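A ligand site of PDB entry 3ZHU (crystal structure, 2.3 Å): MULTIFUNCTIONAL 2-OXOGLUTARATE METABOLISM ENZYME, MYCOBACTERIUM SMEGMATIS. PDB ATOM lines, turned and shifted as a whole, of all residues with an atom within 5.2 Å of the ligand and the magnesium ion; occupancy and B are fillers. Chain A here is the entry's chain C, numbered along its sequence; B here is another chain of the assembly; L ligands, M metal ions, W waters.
The side-chain hydroxyl of Ser 245 sits at hydrogen-bond distance from a ring nitrogen (NE2) of His 661 of chain B.
The backbone NH (N) of Ser 245 lies close to a ring nitrogen (NE2) of His 220 (3.3 Å).
NE2 of Gln 542 of chain B is in hydrogen-bond range of OE2 of Glu 593 of chain B, 2.9 Å away.
OE1 of Glu 593 of chain B lies within hydrogen-bond range of NE2 of Gln 292.
NH2 of Arg 181 lies within hydrogen-bond range of O of His 388, at 3.0 Å.
O of Gln 542 of chain B is in hydrogen-bond range of NE2 of Gln 617 of chain B, at 3.2 Å.
OD2 of Asp 543 of chain B is in hydrogen-bond range of NE2 of Gln 617 of chain B.
The backbone carbonyl oxygen (O) of Leu 591 of chain B is in hydrogen-bond range of the side-chain amide nitrogen (NE2) of Gln 292, at 3.0 Å.
OE1 of Gln 617 of chain B lies close to N1 of the ligand, at 3.3 Å.
Phe 147 touches the ligand.
CE1 of Tyr 219 touches C8 of the ligand (3.4 Å).
CA of His 246 touches N3 of the ligand (3.5 Å).
C of Gly 285 touches O6 of the ligand (3.2 Å).
Gln 292 touches the ligand.
CA of Gly 322 touches O10 of the ligand, at 3.5 Å.
Phe 323 touches the ligand.
Gln 542 of chain B touches the ligand.
Leu 591 of chain B touches the ligand (CD2 to N2, 3.4 Å).
CE1 of Phe 621 of chain B touches N4 of the ligand, 3.4 Å away.
Along chain A the residues within 4 Å of the ligand span positions 147 to 388.
The nearest printed residue that does not touch the ligand is Asp 543 of chain B (4.4 Å).
The magnesium ion is bound by O4 of the ligand, OD1 of Asp 286, O of Ile 321, O5 of the ligand, OD1 of Asn 319 and water W5.
Three residues have an atom within 4 Å of the magnesium ion: Asp 286, Asn 319 and Ile 321.
The nearest printed residue that does not touch the magnesium ion is Gly 322 (4.2 Å).
Water W5 lies within hydrogen-bond range of the backbone carbonyl oxygen of Val 317 (2.6 Å), an oxygen (O9) of the ligand (3.0 Å) and the backbone NH of Asp 286 (3.2 Å).
Water W3 lies within hydrogen-bond range of O2 of the ligand and ND1 of His 180.
Water W6 lies within hydrogen-bond range of OH of Tyr 219, O3 of the ligand and NE2 of His 661 of chain B.
Water W1 lies within hydrogen-bond range of the backbone NH (N) of Phe 323, a ring nitrogen (ND1) of His 388 and an oxygen (O7) of the ligand.
O of Ser 245 sits at hydrogen-bond distance from N4 of the ligand, 2.6 Å away.
An oxygen (O3) of the ligand sits at hydrogen-bond distance from the side-chain hydroxyl (OG) of Ser 245 (2.5 Å).
N2 of the ligand lies within hydrogen-bond range of OE2 of Glu 593 of chain B (2.7 Å).
A ring nitrogen (NE2) of His 661 of chain B is in hydrogen-bond range of an oxygen (O3) of the ligand, at 2.8 Å.
An oxygen (O2) of the ligand lies within hydrogen-bond range of a ring nitrogen (NE2) of His 220 (2.8 Å).
An oxygen (O6) of the ligand is in hydrogen-bond range of the backbone NH (N) of Ala 288.
NE2 of His 180 sits at hydrogen-bond distance from O7 of the ligand, 2.9 Å away.
NH2 of Arg 181 lies within salt-bridge range of O7 of the ligand (3.0 Å).
N of Ala 287 sits at hydrogen-bond distance from O6 of the ligand (3.2 Å).
The backbone NH (N) of Leu 247 is in hydrogen-bond range of a nitrogen (N3) of the ligand.
NE2 of His 388 lies close to S1 of the ligand (3.4 Å).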
ATOM      1  N   PHE A 147     -27.018  -8.387  -9.764  1.00  0.00           N
ATOM      2  CA  PHE A 147     -26.216  -7.490 -10.612  1.00  0.00           C
ATOM      3  C   PHE A 147     -25.561  -6.454  -9.747  1.00  0.00           C
ATOM      4  O   PHE A 147     -25.826  -5.264  -9.882  1.00  0.00           O
ATOM      5  CB  PHE A 147     -27.069  -6.867 -11.750  1.00  0.00           C
ATOM      6  CG  PHE A 147     -27.473  -7.930 -12.748  1.00  0.00           C
ATOM      7  CD1 PHE A 147     -26.554  -8.420 -13.669  1.00  0.00           C
ATOM      8  CD2 PHE A 147     -28.737  -8.524 -12.685  1.00  0.00           C
ATOM      9  CE1 PHE A 147     -26.906  -9.441 -14.547  1.00  0.00           C
ATOM     10  CE2 PHE A 147     -29.080  -9.544 -13.565  1.00  0.00           C
ATOM     11  CZ  PHE A 147     -28.179 -10.001 -14.490  1.00  0.00           C
ATOM     12  N   HIS A 180     -29.760  -2.581 -14.781  1.00  0.00           N
ATOM     13  CA  HIS A 180     -29.607  -3.551 -13.700  1.00  0.00           C
ATOM     14  C   HIS A 180     -28.440  -3.241 -12.715  1.00  0.00           C
ATOM     15  O   HIS A 180     -28.559  -3.561 -11.524  1.00  0.00           O
ATOM     16  CB  HIS A 180     -29.407  -4.960 -14.326  1.00  0.00           C
ATOM     17  CG  HIS A 180     -28.304  -4.948 -15.339  1.00  0.00           C
ATOM     18  ND1 HIS A 180     -28.475  -4.387 -16.587  1.00  0.00           N
ATOM     19  CD2 HIS A 180     -26.994  -5.304 -15.204  1.00  0.00           C
ATOM     20  CE1 HIS A 180     -27.291  -4.446 -17.192  1.00  0.00           C
ATOM     21  NE2 HIS A 180     -26.378  -5.024 -16.402  1.00  0.00           N
ATOM     22  N   ARG A 181     -27.306  -2.662 -13.222  1.00  0.00           N
ATOM     23  CA  ARG A 181     -26.089  -2.451 -12.441  1.00  0.00           C
ATOM     24  C   ARG A 181     -26.327  -1.562 -11.220  1.00  0.00           C
ATOM     25  O   ARG A 181     -26.545  -0.362 -11.371  1.00  0.00           O
ATOM     26  CB  ARG A 181     -24.925  -1.902 -13.302  1.00  0.00           C
ATOM     27  CG  ARG A 181     -23.519  -2.012 -12.658  1.00  0.00           C
ATOM     28  CD  ARG A 181     -23.144  -3.434 -12.221  1.00  0.00           C
ATOM     29  NE  ARG A 181     -23.128  -4.351 -13.353  1.00  0.00           N
ATOM     30  CZ  ARG A 181     -23.055  -5.668 -13.257  1.00  0.00           C
ATOM     31  NH1 ARG A 181     -23.047  -6.259 -12.069  1.00  0.00           N
ATOM     32  NH2 ARG A 181     -23.037  -6.427 -14.354  1.00  0.00           N
ATOM     33  N   VAL A 217     -39.053  -8.968 -12.658  1.00  0.00           N
ATOM     34  CA  VAL A 217     -37.889  -9.234 -11.795  1.00  0.00           C
ATOM     35  C   VAL A 217     -37.589  -8.008 -10.923  1.00  0.00           C
ATOM     36  O   VAL A 217     -37.930  -6.887 -11.304  1.00  0.00           O
ATOM     37  CB  VAL A 217     -36.667  -9.724 -12.609  1.00  0.00           C
ATOM     38  CG1 VAL A 217     -36.938 -11.106 -13.220  1.00  0.00           C
ATOM     39  CG2 VAL A 217     -36.269  -8.713 -13.677  1.00  0.00           C
ATOM     40  N   TYR A 219     -34.908  -6.243 -10.065  1.00  0.00           N
ATOM     41  CA  TYR A 219     -34.071  -5.126 -10.538  1.00  0.00           C
ATOM     42  C   TYR A 219     -34.678  -4.452 -11.845  1.00  0.00           C
ATOM     43  O   TYR A 219     -33.951  -3.989 -12.724  1.00  0.00           O
ATOM     44  CB  TYR A 219     -32.615  -5.577 -10.736  1.00  0.00           C
ATOM     45  CG  TYR A 219     -32.481  -6.941 -11.376  1.00  0.00           C
ATOM     46  CD1 TYR A 219     -32.607  -7.093 -12.749  1.00  0.00           C
ATOM     47  CD2 TYR A 219     -32.227  -8.070 -10.611  1.00  0.00           C
ATOM     48  CE1 TYR A 219     -32.512  -8.349 -13.344  1.00  0.00           C
ATOM     49  CE2 TYR A 219     -32.129  -9.329 -11.197  1.00  0.00           C
ATOM     50  CZ  TYR A 219     -32.269  -9.461 -12.568  1.00  0.00           C
ATOM     51  OH  TYR A 219     -32.138 -10.700 -13.172  1.00  0.00           O
ATOM     52  N   HIS A 220     -36.044  -4.425 -11.921  1.00  0.00           N
ATOM     53  CA  HIS A 220     -36.819  -3.770 -12.964  1.00  0.00           C
ATOM     54  C   HIS A 220     -37.816  -2.841 -12.348  1.00  0.00           C
ATOM     55  O   HIS A 220     -38.390  -2.014 -13.031  1.00  0.00           O
ATOM     56  CB  HIS A 220     -37.551  -4.800 -13.831  1.00  0.00           C
ATOM     57  CG  HIS A 220     -36.706  -5.411 -14.893  1.00  0.00           C
ATOM     58  ND1 HIS A 220     -37.246  -6.292 -15.803  1.00  0.00           N
ATOM     59  CD2 HIS A 220     -35.388  -5.262 -15.155  1.00  0.00           C
ATOM     60  CE1 HIS A 220     -36.241  -6.669 -16.558  1.00  0.00           C
ATOM     61  NE2 HIS A 220     -35.104  -6.063 -16.213  1.00  0.00           N
ATOM     62  N   PRO A 244     -37.859  -2.576 -18.765  1.00  0.00           N
ATOM     63  CA  PRO A 244     -37.592  -3.993 -19.090  1.00  0.00           C
ATOM     64  C   PRO A 244     -36.063  -4.280 -19.063  1.00  0.00           C
ATOM     65  O   PRO A 244     -35.247  -3.392 -18.748  1.00  0.00           O
ATOM     66  CB  PRO A 244     -38.159  -4.101 -20.511  1.00  0.00           C
ATOM     67  CG  PRO A 244     -37.927  -2.724 -21.114  1.00  0.00           C
ATOM     68  CD  PRO A 244     -37.840  -1.734 -19.984  1.00  0.00           C
ATOM     69  N   SER A 245     -35.678  -5.533 -19.453  1.00  0.00           N
ATOM     70  CA  SER A 245     -34.295  -5.976 -19.574  1.00  0.00           C
ATOM     71  C   SER A 245     -33.638  -5.219 -20.690  1.00  0.00           C
ATOM     72  O   SER A 245     -32.455  -4.851 -20.578  1.00  0.00           O
ATOM     73  CB  SER A 245     -34.224  -7.486 -19.834  1.00  0.00           C
ATOM     74  OG  SER A 245     -34.579  -8.292 -18.707  1.00  0.00           O
ATOM     75  N   HIS A 246     -34.430  -4.918 -21.767  1.00  0.00           N
ATOM     76  CA  HIS A 246     -34.039  -4.136 -22.963  1.00  0.00           C
ATOM     77  C   HIS A 246     -33.439  -2.814 -22.527  1.00  0.00           C
ATOM     78  O   HIS A 246     -34.117  -1.853 -22.128  1.00  0.00           O
ATOM     79  CB  HIS A 246     -35.243  -3.906 -23.903  1.00  0.00           C
ATOM     80  CG  HIS A 246     -35.869  -5.177 -24.389  1.00  0.00           C
ATOM     81  ND1 HIS A 246     -36.431  -6.094 -23.506  1.00  0.00           N
ATOM     82  CD2 HIS A 246     -36.029  -5.633 -25.656  1.00  0.00           C
ATOM     83  CE1 HIS A 246     -36.885  -7.088 -24.254  1.00  0.00           C
ATOM     84  NE2 HIS A 246     -36.689  -6.850 -25.552  1.00  0.00           N
ATOM     85  N   LEU A 247     -32.098  -2.854 -22.503  1.00  0.00           N
ATOM     86  CA  LEU A 247     -31.202  -1.791 -22.099  1.00  0.00           C
ATOM     87  C   LEU A 247     -31.401  -0.592 -22.951  1.00  0.00           C
ATOM     88  O   LEU A 247     -31.460  -0.722 -24.205  1.00  0.00           O
ATOM     89  CB  LEU A 247     -29.740  -2.259 -22.225  1.00  0.00           C
ATOM     90  CG  LEU A 247     -29.338  -3.465 -21.376  1.00  0.00           C
ATOM     91  CD1 LEU A 247     -28.017  -4.064 -21.849  1.00  0.00           C
ATOM     92  CD2 LEU A 247     -29.369  -3.143 -19.890  1.00  0.00           C
ATOM     93  N   GLY A 285     -25.005   1.632 -18.727  1.00  0.00           N
ATOM     94  CA  GLY A 285     -23.886   0.706 -18.763  1.00  0.00           C
ATOM     95  C   GLY A 285     -23.035   1.125 -19.945  1.00  0.00           C
ATOM     96  O   GLY A 285     -23.550   1.655 -20.955  1.00  0.00           O
ATOM     97  N   ASP A 286     -21.728   0.946 -19.847  1.00  0.00           N
ATOM     98  CA  ASP A 286     -20.812   1.360 -20.897  1.00  0.00           C
ATOM     99  C   ASP A 286     -21.090   0.659 -22.243  1.00  0.00           C
ATOM    100  O   ASP A 286     -21.035   1.327 -23.291  1.00  0.00           O
ATOM    101  CB  ASP A 286     -19.344   1.186 -20.462  1.00  0.00           C
ATOM    102  CG  ASP A 286     -18.982  -0.218 -19.989  1.00  0.00           C
ATOM    103  OD1 ASP A 286     -19.522  -0.657 -18.949  1.00  0.00           O
ATOM    104  OD2 ASP A 286     -18.140  -0.877 -20.659  1.00  0.00           O
ATOM    105  N   ALA A 287     -21.382  -0.661 -22.254  1.00  0.00           N
ATOM    106  CA  ALA A 287     -21.551  -1.268 -23.574  1.00  0.00           C
ATOM    107  C   ALA A 287     -22.912  -0.895 -24.250  1.00  0.00           C
ATOM    108  O   ALA A 287     -22.961  -0.657 -25.451  1.00  0.00           O
ATOM    109  CB  ALA A 287     -21.380  -2.761 -23.480  1.00  0.00           C
ATOM    110  N   ALA A 288     -23.993  -0.829 -23.456  1.00  0.00           N
ATOM    111  CA  ALA A 288     -25.329  -0.460 -23.928  1.00  0.00           C
ATOM    112  C   ALA A 288     -25.385   1.014 -24.336  1.00  0.00           C
ATOM    113  O   ALA A 288     -26.145   1.343 -25.233  1.00  0.00           O
ATOM    114  CB  ALA A 288     -26.328  -0.720 -22.844  1.00  0.00           C
ATOM    115  N   PHE A 289     -24.595   1.913 -23.700  1.00  0.00           N
ATOM    116  CA  PHE A 289     -24.584   3.334 -24.098  1.00  0.00           C
ATOM    117  C   PHE A 289     -24.002   3.544 -25.479  1.00  0.00           C
ATOM    118  O   PHE A 289     -24.464   4.429 -26.208  1.00  0.00           O
ATOM    119  CB  PHE A 289     -23.814   4.200 -23.113  1.00  0.00           C
ATOM    120  CG  PHE A 289     -24.142   5.670 -23.177  1.00  0.00           C
ATOM    121  CD1 PHE A 289     -25.398   6.141 -22.778  1.00  0.00           C
ATOM    122  CD2 PHE A 289     -23.180   6.602 -23.541  1.00  0.00           C
ATOM    123  CE1 PHE A 289     -25.680   7.506 -22.761  1.00  0.00           C
ATOM    124  CE2 PHE A 289     -23.472   7.968 -23.555  1.00  0.00           C
ATOM    125  CZ  PHE A 289     -24.716   8.412 -23.170  1.00  0.00           C
ATOM    126  N   GLN A 292     -26.605   0.899 -28.312  1.00  0.00           N
ATOM    127  CA  GLN A 292     -28.040   1.072 -28.578  1.00  0.00           C
ATOM    128  C   GLN A 292     -28.362   2.428 -29.221  1.00  0.00           C
ATOM    129  O   GLN A 292     -28.078   3.476 -28.637  1.00  0.00           O
ATOM    130  CB  GLN A 292     -28.864   0.877 -27.278  1.00  0.00           C
ATOM    131  CG  GLN A 292     -28.905  -0.571 -26.788  1.00  0.00           C
ATOM    132  CD  GLN A 292     -29.772  -1.430 -27.674  1.00  0.00           C
ATOM    133  OE1 GLN A 292     -30.958  -1.179 -27.851  1.00  0.00           O
ATOM    134  NE2 GLN A 292     -29.182  -2.473 -28.261  1.00  0.00           N
ATOM    135  N   VAL A 317     -21.961   4.050 -15.789  1.00  0.00           N
ATOM    136  CA  VAL A 317     -21.269   3.169 -14.843  1.00  0.00           C
ATOM    137  C   VAL A 317     -20.357   2.341 -15.728  1.00  0.00           C
ATOM    138  O   VAL A 317     -20.756   1.306 -16.228  1.00  0.00           O
ATOM    139  CB  VAL A 317     -22.264   2.316 -14.004  1.00  0.00           C
ATOM    140  CG1 VAL A 317     -21.535   1.401 -12.994  1.00  0.00           C
ATOM    141  CG2 VAL A 317     -23.273   3.204 -13.286  1.00  0.00           C
ATOM    142  N   ASN A 319     -17.648   0.151 -16.170  1.00  0.00           N
ATOM    143  CA  ASN A 319     -16.865  -0.937 -15.530  1.00  0.00           C
ATOM    144  C   ASN A 319     -16.011  -1.646 -16.587  1.00  0.00           C
ATOM    145  O   ASN A 319     -15.465  -2.713 -16.335  1.00  0.00           O
ATOM    146  CB  ASN A 319     -17.766  -1.921 -14.777  1.00  0.00           C
ATOM    147  CG  ASN A 319     -18.936  -2.469 -15.519  1.00  0.00           C
ATOM    148  OD1 ASN A 319     -19.004  -2.431 -16.764  1.00  0.00           O
ATOM    149  ND2 ASN A 319     -19.896  -3.011 -14.749  1.00  0.00           N
ATOM    150  N   GLN A 320     -15.879  -1.004 -17.743  1.00  0.00           N
ATOM    151  CA  GLN A 320     -15.004  -1.383 -18.868  1.00  0.00           C
ATOM    152  C   GLN A 320     -15.221  -2.844 -19.325  1.00  0.00           C
ATOM    153  O   GLN A 320     -14.277  -3.518 -19.722  1.00  0.00           O
ATOM    154  CB  GLN A 320     -13.544  -1.125 -18.462  1.00  0.00           C
ATOM    155  CG  GLN A 320     -13.344   0.265 -17.831  1.00  0.00           C
ATOM    156  CD  GLN A 320     -11.996   0.436 -17.197  1.00  0.00           C
ATOM    157  OE1 GLN A 320     -10.986   0.494 -17.906  1.00  0.00           O
ATOM    158  NE2 GLN A 320     -11.954   0.513 -15.865  1.00  0.00           N
ATOM    159  N   ILE A 321     -16.488  -3.298 -19.288  1.00  0.00           N
ATOM    160  CA  ILE A 321     -16.892  -4.651 -19.666  1.00  0.00           C
ATOM    161  C   ILE A 321     -18.388  -4.697 -19.990  1.00  0.00           C
ATOM    162  O   ILE A 321     -19.164  -3.989 -19.351  1.00  0.00           O
ATOM    163  CB  ILE A 321     -16.497  -5.671 -18.529  1.00  0.00           C
ATOM    164  CG1 ILE A 321     -16.564  -7.141 -18.992  1.00  0.00           C
ATOM    165  CG2 ILE A 321     -17.254  -5.460 -17.206  1.00  0.00           C
ATOM    166  CD1 ILE A 321     -15.352  -7.571 -19.769  1.00  0.00           C
ATOM    167  N   GLY A 322     -18.760  -5.536 -20.951  1.00  0.00           N
ATOM    168  CA  GLY A 322     -20.134  -5.808 -21.362  1.00  0.00           C
ATOM    169  C   GLY A 322     -20.336  -7.308 -21.339  1.00  0.00           C
ATOM    170  O   GLY A 322     -20.154  -7.976 -22.365  1.00  0.00           O
ATOM    171  N   PHE A 323     -20.638  -7.863 -20.129  1.00  0.00           N
ATOM    172  CA  PHE A 323     -20.761  -9.307 -19.855  1.00  0.00           C
ATOM    173  C   PHE A 323     -19.369  -9.989 -20.159  1.00  0.00           C
ATOM    174  O   PHE A 323     -18.489  -9.941 -19.294  1.00  0.00           O
ATOM    175  CB  PHE A 323     -21.948  -9.929 -20.629  1.00  0.00           C
ATOM    176  CG  PHE A 323     -22.392 -11.324 -20.232  1.00  0.00           C
ATOM    177  CD1 PHE A 323     -21.603 -12.122 -19.396  1.00  0.00           C
ATOM    178  CD2 PHE A 323     -23.570 -11.869 -20.765  1.00  0.00           C
ATOM    179  CE1 PHE A 323     -22.002 -13.405 -19.055  1.00  0.00           C
ATOM    180  CE2 PHE A 323     -23.965 -13.164 -20.419  1.00  0.00           C
ATOM    181  CZ  PHE A 323     -23.198 -13.911 -19.555  1.00  0.00           C
ATOM    182  N   HIS A 388     -20.484 -11.123 -14.540  1.00  0.00           N
ATOM    183  CA  HIS A 388     -21.575 -10.311 -15.081  1.00  0.00           C
ATOM    184  C   HIS A 388     -22.812 -10.364 -14.178  1.00  0.00           C
ATOM    185  O   HIS A 388     -23.411  -9.324 -13.884  1.00  0.00           O
ATOM    186  CB  HIS A 388     -21.927 -10.735 -16.487  1.00  0.00           C
ATOM    187  CG  HIS A 388     -23.049  -9.941 -17.068  1.00  0.00           C
ATOM    188  ND1 HIS A 388     -22.991  -8.559 -17.146  1.00  0.00           N
ATOM    189  CD2 HIS A 388     -24.258 -10.350 -17.515  1.00  0.00           C
ATOM    190  CE1 HIS A 388     -24.141  -8.180 -17.665  1.00  0.00           C
ATOM    191  NE2 HIS A 388     -24.936  -9.224 -17.909  1.00  0.00           N
ATOM    192  N   GLN B 542     -24.125 -11.392 -29.233  1.00  0.00           N
ATOM    193  CA  GLN B 542     -23.696 -10.926 -27.921  1.00  0.00           C
ATOM    194  C   GLN B 542     -23.129 -12.073 -27.058  1.00  0.00           C
ATOM    195  O   GLN B 542     -23.837 -13.015 -26.707  1.00  0.00           O
ATOM    196  CB  GLN B 542     -24.852 -10.201 -27.227  1.00  0.00           C
ATOM    197  CG  GLN B 542     -24.996  -8.744 -27.687  1.00  0.00           C
ATOM    198  CD  GLN B 542     -26.431  -8.250 -27.595  1.00  0.00           C
ATOM    199  OE1 GLN B 542     -27.213  -8.693 -26.745  1.00  0.00           O
ATOM    200  NE2 GLN B 542     -26.809  -7.312 -28.497  1.00  0.00           N
ATOM    201  N   ASP B 543     -21.806 -12.005 -26.794  1.00  0.00           N
ATOM    202  CA  ASP B 543     -21.049 -12.992 -26.004  1.00  0.00           C
ATOM    203  C   ASP B 543     -21.117 -14.385 -26.689  1.00  0.00           C
ATOM    204  O   ASP B 543     -21.133 -15.431 -26.013  1.00  0.00           O
ATOM    205  CB  ASP B 543     -21.600 -13.032 -24.560  1.00  0.00           C
ATOM    206  CG  ASP B 543     -21.614 -11.651 -23.939  1.00  0.00           C
ATOM    207  OD1 ASP B 543     -20.523 -11.132 -23.655  1.00  0.00           O
ATOM    208  OD2 ASP B 543     -22.719 -11.037 -23.877  1.00  0.00           O
ATOM    209  N   LEU B 591     -23.270  -4.181 -28.460  1.00  0.00           N
ATOM    210  CA  LEU B 591     -24.566  -4.379 -27.827  1.00  0.00           C
ATOM    211  C   LEU B 591     -25.655  -3.687 -28.663  1.00  0.00           C
ATOM    212  O   LEU B 591     -26.181  -2.638 -28.270  1.00  0.00           O
ATOM    213  CB  LEU B 591     -24.527  -3.883 -26.384  1.00  0.00           C
ATOM    214  CG  LEU B 591     -25.320  -4.689 -25.357  1.00  0.00           C
ATOM    215  CD1 LEU B 591     -24.901  -4.291 -23.986  1.00  0.00           C
ATOM    216  CD2 LEU B 591     -26.844  -4.549 -25.555  1.00  0.00           C
ATOM    217  N   GLU B 593     -28.960  -4.852 -31.783  1.00  0.00           N
ATOM    218  CA  GLU B 593     -29.767  -5.871 -32.445  1.00  0.00           C
ATOM    219  C   GLU B 593     -30.056  -5.414 -33.857  1.00  0.00           C
ATOM    220  O   GLU B 593     -29.762  -6.158 -34.785  1.00  0.00           O
ATOM    221  CB  GLU B 593     -31.077  -6.173 -31.687  1.00  0.00           C
ATOM    222  CG  GLU B 593     -30.855  -6.965 -30.419  1.00  0.00           C
ATOM    223  CD  GLU B 593     -30.366  -6.168 -29.223  1.00  0.00           C
ATOM    224  OE1 GLU B 593     -30.641  -4.948 -29.139  1.00  0.00           O
ATOM    225  OE2 GLU B 593     -29.692  -6.769 -28.360  1.00  0.00           O
ATOM    226  N   GLN B 617     -28.915 -12.850 -27.503  1.00  0.00           N
ATOM    227  CA  GLN B 617     -28.549 -13.247 -26.146  1.00  0.00           C
ATOM    228  C   GLN B 617     -29.683 -14.141 -25.631  1.00  0.00           C
ATOM    229  O   GLN B 617     -29.454 -15.268 -25.173  1.00  0.00           O
ATOM    230  CB  GLN B 617     -28.352 -11.996 -25.247  1.00  0.00           C
ATOM    231  CG  GLN B 617     -27.927 -12.299 -23.820  1.00  0.00           C
ATOM    232  CD  GLN B 617     -26.536 -11.807 -23.551  1.00  0.00           C
ATOM    233  OE1 GLN B 617     -26.331 -10.832 -22.825  1.00  0.00           O
ATOM    234  NE2 GLN B 617     -25.541 -12.458 -24.107  1.00  0.00           N
ATOM    235  N   PHE B 618     -30.900 -13.625 -25.777  1.00  0.00           N
ATOM    236  CA  PHE B 618     -32.192 -14.244 -25.518  1.00  0.00           C
ATOM    237  C   PHE B 618     -33.053 -13.732 -26.649  1.00  0.00           C
ATOM    238  O   PHE B 618     -32.856 -12.599 -27.079  1.00  0.00           O
ATOM    239  CB  PHE B 618     -32.758 -13.891 -24.116  1.00  0.00           C
ATOM    240  CG  PHE B 618     -32.020 -14.462 -22.936  1.00  0.00           C
ATOM    241  CD1 PHE B 618     -30.907 -13.803 -22.404  1.00  0.00           C
ATOM    242  CD2 PHE B 618     -32.486 -15.594 -22.285  1.00  0.00           C
ATOM    243  CE1 PHE B 618     -30.223 -14.327 -21.299  1.00  0.00           C
ATOM    244  CE2 PHE B 618     -31.823 -16.093 -21.163  1.00  0.00           C
ATOM    245  CZ  PHE B 618     -30.709 -15.460 -20.674  1.00  0.00           C
ATOM    246  N   PHE B 621     -34.904 -10.114 -27.187  1.00  0.00           N
ATOM    247  CA  PHE B 621     -34.256  -8.876 -27.644  1.00  0.00           C
ATOM    248  C   PHE B 621     -34.240  -8.717 -29.150  1.00  0.00           C
ATOM    249  O   PHE B 621     -33.862  -7.644 -29.617  1.00  0.00           O
ATOM    250  CB  PHE B 621     -32.813  -8.767 -27.082  1.00  0.00           C
ATOM    251  CG  PHE B 621     -32.741  -8.912 -25.594  1.00  0.00           C
ATOM    252  CD1 PHE B 621     -33.374  -8.005 -24.756  1.00  0.00           C
ATOM    253  CD2 PHE B 621     -32.038  -9.961 -25.010  1.00  0.00           C
ATOM    254  CE1 PHE B 621     -33.317  -8.132 -23.369  1.00  0.00           C
ATOM    255  CE2 PHE B 621     -31.981 -10.098 -23.627  1.00  0.00           C
ATOM    256  CZ  PHE B 621     -32.624  -9.180 -22.815  1.00  0.00           C
ATOM    257  N   HIS B 661     -36.764 -12.925 -20.487  1.00  0.00           N
ATOM    258  CA  HIS B 661     -35.763 -13.977 -20.603  1.00  0.00           C
ATOM    259  C   HIS B 661     -36.458 -15.280 -20.858  1.00  0.00           C
ATOM    260  O   HIS B 661     -36.018 -16.339 -20.401  1.00  0.00           O
ATOM    261  CB  HIS B 661     -34.896 -14.016 -19.333  1.00  0.00           C
ATOM    262  CG  HIS B 661     -33.962 -12.846 -19.245  1.00  0.00           C
ATOM    263  ND1 HIS B 661     -32.675 -12.912 -19.733  1.00  0.00           N
ATOM    264  CD2 HIS B 661     -34.171 -11.603 -18.746  1.00  0.00           C
ATOM    265  CE1 HIS B 661     -32.128 -11.725 -19.509  1.00  0.00           C
ATOM    266  NE2 HIS B 661     -32.987 -10.913 -18.901  1.00  0.00           N
HETATM  267  S1  LIG L   1     -26.801  -7.036 -19.680  1.00  0.00           S
HETATM  268  C1  LIG L   1     -28.141  -7.711 -20.562  1.00  0.00           C
HETATM  269  N1  LIG L   1     -27.797  -7.995 -21.850  1.00  0.00           N
HETATM  270  C2  LIG L   1     -26.497  -7.676 -22.166  1.00  0.00           C
HETATM  271  C3  LIG L   1     -25.725  -7.137 -21.008  1.00  0.00           C
HETATM  272  C4  LIG L   1     -29.127  -8.350 -19.635  1.00  0.00           C
HETATM  273  C5  LIG L   1     -29.876  -7.361 -18.777  1.00  0.00           C
HETATM  274  O1  LIG L   1     -29.842  -9.391 -20.092  1.00  0.00           O
HETATM  275  P1  LIG L   1     -23.094  -2.943 -20.001  1.00  0.00           P
HETATM  276  P2  LIG L   1     -22.945  -3.754 -17.153  1.00  0.00           P
HETATM  277  N2  LIG L   1     -29.799  -6.295 -25.694  1.00  0.00           N
HETATM  278  C6  LIG L   1     -29.593  -7.600 -17.317  1.00  0.00           C
HETATM  279  O2  LIG L   1     -32.399  -6.804 -16.558  1.00  0.00           O
HETATM  280  C7  LIG L   1     -30.636  -8.459 -16.631  1.00  0.00           C
HETATM  281  O3  LIG L   1     -32.922  -8.906 -16.997  1.00  0.00           O
HETATM  282  C8  LIG L   1     -32.085  -8.013 -16.745  1.00  0.00           C
HETATM  283  O4  LIG L   1     -21.595  -2.742 -19.905  1.00  0.00           O
HETATM  284  O5  LIG L   1     -21.471  -3.747 -17.415  1.00  0.00           O
HETATM  285  C9  LIG L   1     -30.618  -5.386 -25.135  1.00  0.00           C
HETATM  286  C10 LIG L   1     -31.222  -4.275 -25.939  1.00  0.00           C
HETATM  287  O6  LIG L   1     -23.926  -1.882 -20.745  1.00  0.00           O
HETATM  288  O7  LIG L   1     -23.523  -5.129 -16.991  1.00  0.00           O
HETATM  289  N3  LIG L   1     -30.913  -5.475 -23.822  1.00  0.00           N
HETATM  290  C11 LIG L   1     -28.800  -8.517 -22.819  1.00  0.00           C
HETATM  291  O8  LIG L   1     -23.707  -3.190 -18.507  1.00  0.00           O
HETATM  292  O9  LIG L   1     -23.295  -2.733 -16.065  1.00  0.00           O
HETATM  293  C12 LIG L   1     -30.386  -6.477 -23.060  1.00  0.00           C
HETATM  294  N4  LIG L   1     -30.803  -6.513 -21.793  1.00  0.00           N
HETATM  295  C13 LIG L   1     -25.831  -7.903 -23.516  1.00  0.00           C
HETATM  296  C14 LIG L   1     -29.497  -7.397 -23.607  1.00  0.00           C
HETATM  297  C15 LIG L   1     -24.303  -6.638 -20.806  1.00  0.00           C
HETATM  298  C16 LIG L   1     -24.402  -5.159 -20.421  1.00  0.00           C
HETATM  299  O10 LIG L   1     -23.270  -4.343 -20.793  1.00  0.00           O
HETATM  300  C17 LIG L   1     -29.227  -7.258 -24.970  1.00  0.00           C
HETATM  301 MG    MG M   1     -20.244  -2.478 -18.476  1.00  0.00          MG
HETATM  302  O   HOH W   1     -21.029  -6.721 -17.808  1.00  0.00           O
HETATM  303  O   HOH W   2     -25.318  -1.275 -16.486  1.00  0.00           O
HETATM  304  O   HOH W   3     -31.627  -4.322 -16.840  1.00  0.00           O
HETATM  305  O   HOH W   4     -26.156  -1.673 -19.284  1.00  0.00           O
HETATM  306  O   HOH W   5     -21.256  -0.991 -17.340  1.00  0.00           O
HETATM  307  O   HOH W   6     -32.162 -11.168 -15.578  1.00  0.00           O
